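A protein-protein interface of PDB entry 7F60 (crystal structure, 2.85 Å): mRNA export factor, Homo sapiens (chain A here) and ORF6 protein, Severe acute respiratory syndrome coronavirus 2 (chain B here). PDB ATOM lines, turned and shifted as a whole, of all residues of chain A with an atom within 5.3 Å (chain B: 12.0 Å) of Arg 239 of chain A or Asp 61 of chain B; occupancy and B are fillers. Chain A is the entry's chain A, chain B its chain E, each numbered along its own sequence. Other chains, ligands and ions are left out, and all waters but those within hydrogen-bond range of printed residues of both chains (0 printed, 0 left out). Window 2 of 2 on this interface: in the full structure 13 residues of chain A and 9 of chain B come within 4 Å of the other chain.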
ATOM      1  N   LEU A 211      -0.844   3.753  32.223  1.00  0.00           N
ATOM      2  CA  LEU A 211       0.129   4.831  32.249  1.00  0.00           C
ATOM      3  C   LEU A 211       1.013   4.674  33.479  1.00  0.00           C
ATOM      4  O   LEU A 211       0.561   4.209  34.530  1.00  0.00           O
ATOM      5  CB  LEU A 211      -0.556   6.203  32.261  1.00  0.00           C
ATOM      6  CG  LEU A 211      -1.529   6.487  31.114  1.00  0.00           C
ATOM      7  CD1 LEU A 211      -2.224   7.826  31.314  1.00  0.00           C
ATOM      8  CD2 LEU A 211      -0.809   6.450  29.775  1.00  0.00           C
ATOM      9  N   LEU A 233      -7.812   8.157  29.943  1.00  0.00           N
ATOM     10  CA  LEU A 233      -7.015   8.520  31.108  1.00  0.00           C
ATOM     11  C   LEU A 233      -5.832   9.380  30.684  1.00  0.00           C
ATOM     12  O   LEU A 233      -5.121   9.037  29.731  1.00  0.00           O
ATOM     13  CB  LEU A 233      -6.521   7.268  31.833  1.00  0.00           C
ATOM     14  CG  LEU A 233      -5.610   7.471  33.045  1.00  0.00           C
ATOM     15  CD1 LEU A 233      -6.284   8.362  34.071  1.00  0.00           C
ATOM     16  CD2 LEU A 233      -5.236   6.133  33.659  1.00  0.00           C
ATOM     17  N   GLY A 234      -5.617  10.489  31.398  1.00  0.00           N
ATOM     18  CA  GLY A 234      -4.489  11.363  31.115  1.00  0.00           C
ATOM     19  C   GLY A 234      -3.533  11.557  32.281  1.00  0.00           C
ATOM     20  O   GLY A 234      -3.965  11.771  33.418  1.00  0.00           O
ATOM     21  N   SER A 235      -2.231  11.502  32.012  1.00  0.00           N
ATOM     22  CA  SER A 235      -1.205  11.635  33.038  1.00  0.00           C
ATOM     23  C   SER A 235      -0.474  12.970  32.891  1.00  0.00           C
ATOM     24  O   SER A 235      -0.827  13.820  32.068  1.00  0.00           O
ATOM     25  CB  SER A 235      -0.226  10.455  32.987  1.00  0.00           C
ATOM     26  OG  SER A 235       0.549  10.443  31.801  1.00  0.00           O
ATOM     27  N   GLU A 237       2.539  13.164  32.076  1.00  0.00           N
ATOM     28  CA  GLU A 237       3.646  12.833  31.185  1.00  0.00           C
ATOM     29  C   GLU A 237       3.254  12.948  29.713  1.00  0.00           C
ATOM     30  O   GLU A 237       3.731  12.183  28.871  1.00  0.00           O
ATOM     31  CB  GLU A 237       4.167  11.432  31.487  1.00  0.00           C
ATOM     32  CG  GLU A 237       5.589  11.194  31.026  1.00  0.00           C
ATOM     33  CD  GLU A 237       5.709   9.951  30.178  1.00  0.00           C
ATOM     34  OE1 GLU A 237       4.820   9.078  30.269  1.00  0.00           O
ATOM     35  OE2 GLU A 237       6.687   9.850  29.411  1.00  0.00           O
ATOM     36  N   GLY A 238       2.405  13.919  29.387  1.00  0.00           N
ATOM     37  CA  GLY A 238       2.018  14.149  27.997  1.00  0.00           C
ATOM     38  C   GLY A 238       1.517  12.899  27.285  1.00  0.00           C
ATOM     39  O   GLY A 238       1.790  12.710  26.098  1.00  0.00           O
ATOM     40  N   ARG A 239       0.782  12.062  28.007  1.00  0.00           N
ATOM     41  CA  ARG A 239       0.363  10.760  27.511  1.00  0.00           C
ATOM     42  C   ARG A 239      -1.074  10.524  27.938  1.00  0.00           C
ATOM     43  O   ARG A 239      -1.435  10.774  29.091  1.00  0.00           O
ATOM     44  CB  ARG A 239       1.270   9.651  28.048  1.00  0.00           C
ATOM     45  CG  ARG A 239       1.216   8.375  27.251  1.00  0.00           C
ATOM     46  CD  ARG A 239       2.190   7.353  27.798  1.00  0.00           C
ATOM     47  NE  ARG A 239       3.577   7.798  27.699  1.00  0.00           N
ATOM     48  CZ  ARG A 239       4.372   7.535  26.668  1.00  0.00           C
ATOM     49  NH1 ARG A 239       3.920   6.829  25.642  1.00  0.00           N
ATOM     50  NH2 ARG A 239       5.623   7.978  26.664  1.00  0.00           N
ATOM     51  N   VAL A 240      -1.889  10.060  26.995  1.00  0.00           N
ATOM     52  CA  VAL A 240      -3.293   9.754  27.236  1.00  0.00           C
ATOM     53  C   VAL A 240      -3.559   8.324  26.789  1.00  0.00           C
ATOM     54  O   VAL A 240      -3.129   7.912  25.707  1.00  0.00           O
ATOM     55  CB  VAL A 240      -4.226  10.738  26.502  1.00  0.00           C
ATOM     56  CG1 VAL A 240      -5.670  10.286  26.610  1.00  0.00           C
ATOM     57  CG2 VAL A 240      -4.065  12.137  27.070  1.00  0.00           C
ATOM     58  N   ALA A 241      -4.269   7.572  27.626  1.00  0.00           N
ATOM     59  CA  ALA A 241      -4.592   6.178  27.364  1.00  0.00           C
ATOM     60  C   ALA A 241      -6.070   6.031  27.029  1.00  0.00           C
ATOM     61  O   ALA A 241      -6.920   6.708  27.616  1.00  0.00           O
ATOM     62  CB  ALA A 241      -4.245   5.303  28.570  1.00  0.00           C
ATOM     63  N   PHE A 255      -5.078   1.303  23.535  1.00  0.00           N
ATOM     64  CA  PHE A 255      -3.822   1.895  23.103  1.00  0.00           C
ATOM     65  C   PHE A 255      -3.509   3.115  23.957  1.00  0.00           C
ATOM     66  O   PHE A 255      -4.333   3.579  24.751  1.00  0.00           O
ATOM     67  CB  PHE A 255      -3.860   2.275  21.615  1.00  0.00           C
ATOM     68  CG  PHE A 255      -4.923   3.284  21.266  1.00  0.00           C
ATOM     69  CD1 PHE A 255      -4.644   4.642  21.271  1.00  0.00           C
ATOM     70  CD2 PHE A 255      -6.200   2.871  20.919  1.00  0.00           C
ATOM     71  CE1 PHE A 255      -5.620   5.569  20.948  1.00  0.00           C
ATOM     72  CE2 PHE A 255      -7.180   3.794  20.594  1.00  0.00           C
ATOM     73  CZ  PHE A 255      -6.889   5.143  20.607  1.00  0.00           C
ATOM     74  N   THR A 256      -2.295   3.631  23.774  1.00  0.00           N
ATOM     75  CA  THR A 256      -1.818   4.824  24.455  1.00  0.00           C
ATOM     76  C   THR A 256      -1.104   5.699  23.435  1.00  0.00           C
ATOM     77  O   THR A 256      -0.391   5.187  22.565  1.00  0.00           O
ATOM     78  CB  THR A 256      -0.889   4.452  25.627  1.00  0.00           C
ATOM     79  OG1 THR A 256      -1.545   4.727  26.870  1.00  0.00           O
ATOM     80  CG2 THR A 256       0.424   5.216  25.571  1.00  0.00           C
ATOM     81  N   PHE A 257      -1.315   7.011  23.520  1.00  0.00           N
ATOM     82  CA  PHE A 257      -0.726   7.929  22.557  1.00  0.00           C
ATOM     83  C   PHE A 257      -0.145   9.141  23.271  1.00  0.00           C
ATOM     84  O   PHE A 257      -0.585   9.515  24.361  1.00  0.00           O
ATOM     85  CB  PHE A 257      -1.743   8.377  21.493  1.00  0.00           C
ATOM     86  CG  PHE A 257      -2.861   9.230  22.028  1.00  0.00           C
ATOM     87  CD1 PHE A 257      -2.753  10.613  22.041  1.00  0.00           C
ATOM     88  CD2 PHE A 257      -4.029   8.650  22.496  1.00  0.00           C
ATOM     89  CE1 PHE A 257      -3.782  11.399  22.526  1.00  0.00           C
ATOM     90  CE2 PHE A 257      -5.061   9.432  22.981  1.00  0.00           C
ATOM     91  CZ  PHE A 257      -4.938  10.808  22.995  1.00  0.00           C
ATOM     92  N   LYS A 258       0.852   9.747  22.636  1.00  0.00           N
ATOM     93  CA  LYS A 258       1.521  10.934  23.144  1.00  0.00           C
ATOM     94  C   LYS A 258       0.761  12.187  22.731  1.00  0.00           C
ATOM     95  O   LYS A 258       0.037  12.203  21.732  1.00  0.00           O
ATOM     96  CB  LYS A 258       2.959  11.005  22.629  1.00  0.00           C
ATOM     97  CG  LYS A 258       3.810   9.787  22.963  1.00  0.00           C
ATOM     98  CD  LYS A 258       5.123   9.805  22.191  1.00  0.00           C
ATOM     99  CE  LYS A 258       6.013   8.630  22.576  1.00  0.00           C
ATOM    100  NZ  LYS A 258       7.253   8.595  21.749  1.00  0.00           N
ATOM    101  N   CYS A 259       0.945  13.252  23.509  1.00  0.00           N
ATOM    102  CA  CYS A 259       0.261  14.513  23.252  1.00  0.00           C
ATOM    103  C   CYS A 259       0.891  15.606  24.105  1.00  0.00           C
ATOM    104  O   CYS A 259       1.576  15.328  25.093  1.00  0.00           O
ATOM    105  CB  CYS A 259      -1.237  14.409  23.549  1.00  0.00           C
ATOM    106  SG  CYS A 259      -1.616  13.908  25.240  1.00  0.00           S
ATOM    107  N   ARG A 261       3.333  17.870  23.712  1.00  0.00           N
ATOM    108  CA  ARG A 261       4.789  17.870  23.801  1.00  0.00           C
ATOM    109  C   ARG A 261       5.329  18.801  22.727  1.00  0.00           C
ATOM    110  O   ARG A 261       5.157  18.538  21.533  1.00  0.00           O
ATOM    111  CB  ARG A 261       5.353  16.458  23.629  1.00  0.00           C
ATOM    112  CG  ARG A 261       4.928  15.480  24.712  1.00  0.00           C
ATOM    113  CD  ARG A 261       4.671  14.100  24.128  1.00  0.00           C
ATOM    114  NE  ARG A 261       4.763  13.051  25.137  1.00  0.00           N
ATOM    115  CZ  ARG A 261       5.877  12.376  25.406  1.00  0.00           C
ATOM    116  NH1 ARG A 261       6.990  12.642  24.736  1.00  0.00           N
ATOM    117  NH2 ARG A 261       5.880  11.435  26.340  1.00  0.00           N
ATOM    118  N   VAL A 276      -1.113  16.749  31.050  1.00  0.00           N
ATOM    119  CA  VAL A 276      -2.493  16.835  30.578  1.00  0.00           C
ATOM    120  C   VAL A 276      -3.368  17.267  31.748  1.00  0.00           C
ATOM    121  O   VAL A 276      -3.479  16.552  32.749  1.00  0.00           O
ATOM    122  CB  VAL A 276      -2.965  15.494  29.997  1.00  0.00           C
ATOM    123  CG1 VAL A 276      -4.322  15.654  29.328  1.00  0.00           C
ATOM    124  CG2 VAL A 276      -1.938  14.947  29.018  1.00  0.00           C
ATOM    125  N   PRO B  57      -1.845  11.388  11.657  1.00  0.00           N
ATOM    126  CA  PRO B  57      -2.055  10.123  12.377  1.00  0.00           C
ATOM    127  C   PRO B  57      -1.507  10.174  13.798  1.00  0.00           C
ATOM    128  O   PRO B  57      -0.521  10.854  14.081  1.00  0.00           O
ATOM    129  CB  PRO B  57      -1.300   9.104  11.514  1.00  0.00           C
ATOM    130  CG  PRO B  57      -0.260   9.923  10.776  1.00  0.00           C
ATOM    131  CD  PRO B  57      -0.881  11.268  10.550  1.00  0.00           C
ATOM    132  N   MET B  58      -2.147   9.429  14.698  1.00  0.00           N
ATOM    133  CA  MET B  58      -1.759   9.487  16.103  1.00  0.00           C
ATOM    134  C   MET B  58      -0.387   8.862  16.321  1.00  0.00           C
ATOM    135  O   MET B  58       0.028   7.950  15.605  1.00  0.00           O
ATOM    136  CB  MET B  58      -2.789   8.780  16.983  1.00  0.00           C
ATOM    137  CG  MET B  58      -3.782   9.707  17.655  1.00  0.00           C
ATOM    138  SD  MET B  58      -4.835   8.735  18.740  1.00  0.00           S
ATOM    139  CE  MET B  58      -6.006   9.969  19.289  1.00  0.00           C
ATOM    140  N   GLU B  59       0.328   9.375  17.322  1.00  0.00           N
ATOM    141  CA  GLU B  59       1.602   8.787  17.734  1.00  0.00           C
ATOM    142  C   GLU B  59       1.285   7.827  18.874  1.00  0.00           C
ATOM    143  O   GLU B  59       1.247   8.211  20.043  1.00  0.00           O
ATOM    144  CB  GLU B  59       2.605   9.860  18.147  1.00  0.00           C
ATOM    145  CG  GLU B  59       2.412  11.218  17.503  1.00  0.00           C
ATOM    146  CD  GLU B  59       1.399  12.069  18.237  1.00  0.00           C
ATOM    147  OE1 GLU B  59       0.575  11.494  18.981  1.00  0.00           O
ATOM    148  OE2 GLU B  59       1.434  13.307  18.088  1.00  0.00           O
ATOM    149  N   ILE B  60       1.049   6.561  18.525  1.00  0.00           N
ATOM    150  CA  ILE B  60       0.580   5.541  19.462  1.00  0.00           C
ATOM    151  C   ILE B  60       1.706   4.561  19.764  1.00  0.00           C
ATOM    152  O   ILE B  60       2.530   4.240  18.901  1.00  0.00           O
ATOM    153  CB  ILE B  60      -0.665   4.807  18.904  1.00  0.00           C
ATOM    154  CG1 ILE B  60      -0.655   3.300  19.230  1.00  0.00           C
ATOM    155  CG2 ILE B  60      -0.820   5.071  17.404  1.00  0.00           C
ATOM    156  CD1 ILE B  60      -0.204   2.390  18.092  1.00  0.00           C
ATOM    157  N   ASP B  61       1.723   4.074  21.004  1.00  0.00           N
ATOM    158  CA  ASP B  61       2.681   3.071  21.452  1.00  0.00           C
ATOM    159  C   ASP B  61       2.082   1.667  21.366  1.00  0.00           C
ATOM    160  O   ASP B  61       0.962   1.429  21.820  1.00  0.00           O
ATOM    161  CB  ASP B  61       3.113   3.381  22.884  1.00  0.00           C
ATOM    162  CG  ASP B  61       3.506   4.836  23.062  1.00  0.00           C
ATOM    163  OD1 ASP B  61       4.714   5.140  22.980  1.00  0.00           O
ATOM    164  OD2 ASP B  61       2.603   5.683  23.247  1.00  0.00           O
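N of Phe 257 of chain A sits at hydrogen-bond distance from O of Val 240 of chain A, at 3.0 Å. O of Arg 239 of chain A is in hydrogen-bond range of OG of Ser 235 of chain A, 3.4 Å away. The side-chain carboxylate (OE1) of Glu 237 of chain A is in salt-bridge range of the guanidinium group (NE) of Arg 239 of chain A, 3.1 Å away.
Among the printed residues, merely in contact across the chains: Phe 255 of chain A with Met 58 of chain B, Thr 256 of chain A with Ile 60 of chain B, Phe 257 of chain A with Met 58 of chain B, Phe 257 of chain A with Glu 59 of chain B and Lys 258 of chain A with Asp 61 of chain B.
Of the 16 printed residues of chain A, 5 touch a printed residue of chain B. Hydrophobic or aromatic side chains of chain A within 4 Å of the printed part of chain B: Phe 255 and Phe 257. Along chain A the printed residues that touch a printed residue of chain B span positions 239 to 258. Of the 5 printed residues of chain B, 4 touch a printed residue of chain A. Among the printed residues, 8 pairs touch across the chains.
N of Lys 258 of chain A sits at hydrogen-bond distance from O of Glu 59 of chain B (3.0 Å). NH1 of Arg 239 of chain A lies within salt-bridge range of OD2 of Asp 61 of chain B, at 3.0 Å. The backbone carbonyl oxygen (O) of Thr 256 of chain A lies within hydrogen-bond range of the backbone NH (N) of Asp 61 of chain B, 2.9 Å away.
Of the printed residues of chain B, Arg 239 of chain A touches Asp 61. Asp 61 of chain B touches three residues of chain A. No residue of chain B comes within 4 Å of Leu 211 of chain A. No residue of chain B comes within 4 Å of Leu 233 of chain A. No residue of chain B comes within 4 Å of Ser 235 of chain A. No residue of chain B comes within 4 Å of Glu 237 of chain A. No residue of chain B comes within 4 Å of Ala 241 of chain A. Of chain B, only Ile 60 and Asp 61 come within 4 Å of Thr 256 of chain A. Of the printed residues of chain B, Phe 257 of chain A touches Met 58 and Glu 59. Cys 259 of chain A touches none of the printed residues of chain B. No residue of chain B comes within 4 Å of Val 276 of chain A. Printed residues of chain A within 4 Å of Met 58 of chain B: Phe 255 (3.9 Å) and Phe 257 (3.8 Å). Of the printed residues of chain A, Glu 59 of chain B touches Phe 257 and Lys 258. Of the printed residues of chain B, Phe 255 of chain A touches Met 58. The nearest residue of chain B that does not touch Arg 239 of chain A is Glu 59 of chain B (6.4 Å). The nearest residue of chain A that does not touch Asp 61 of chain B is Phe 257 of chain A (4.1 Å). The nearest printed residue of chain B that does not touch Phe 255 of chain A is Ile 60 of chain B (4.1 Å).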
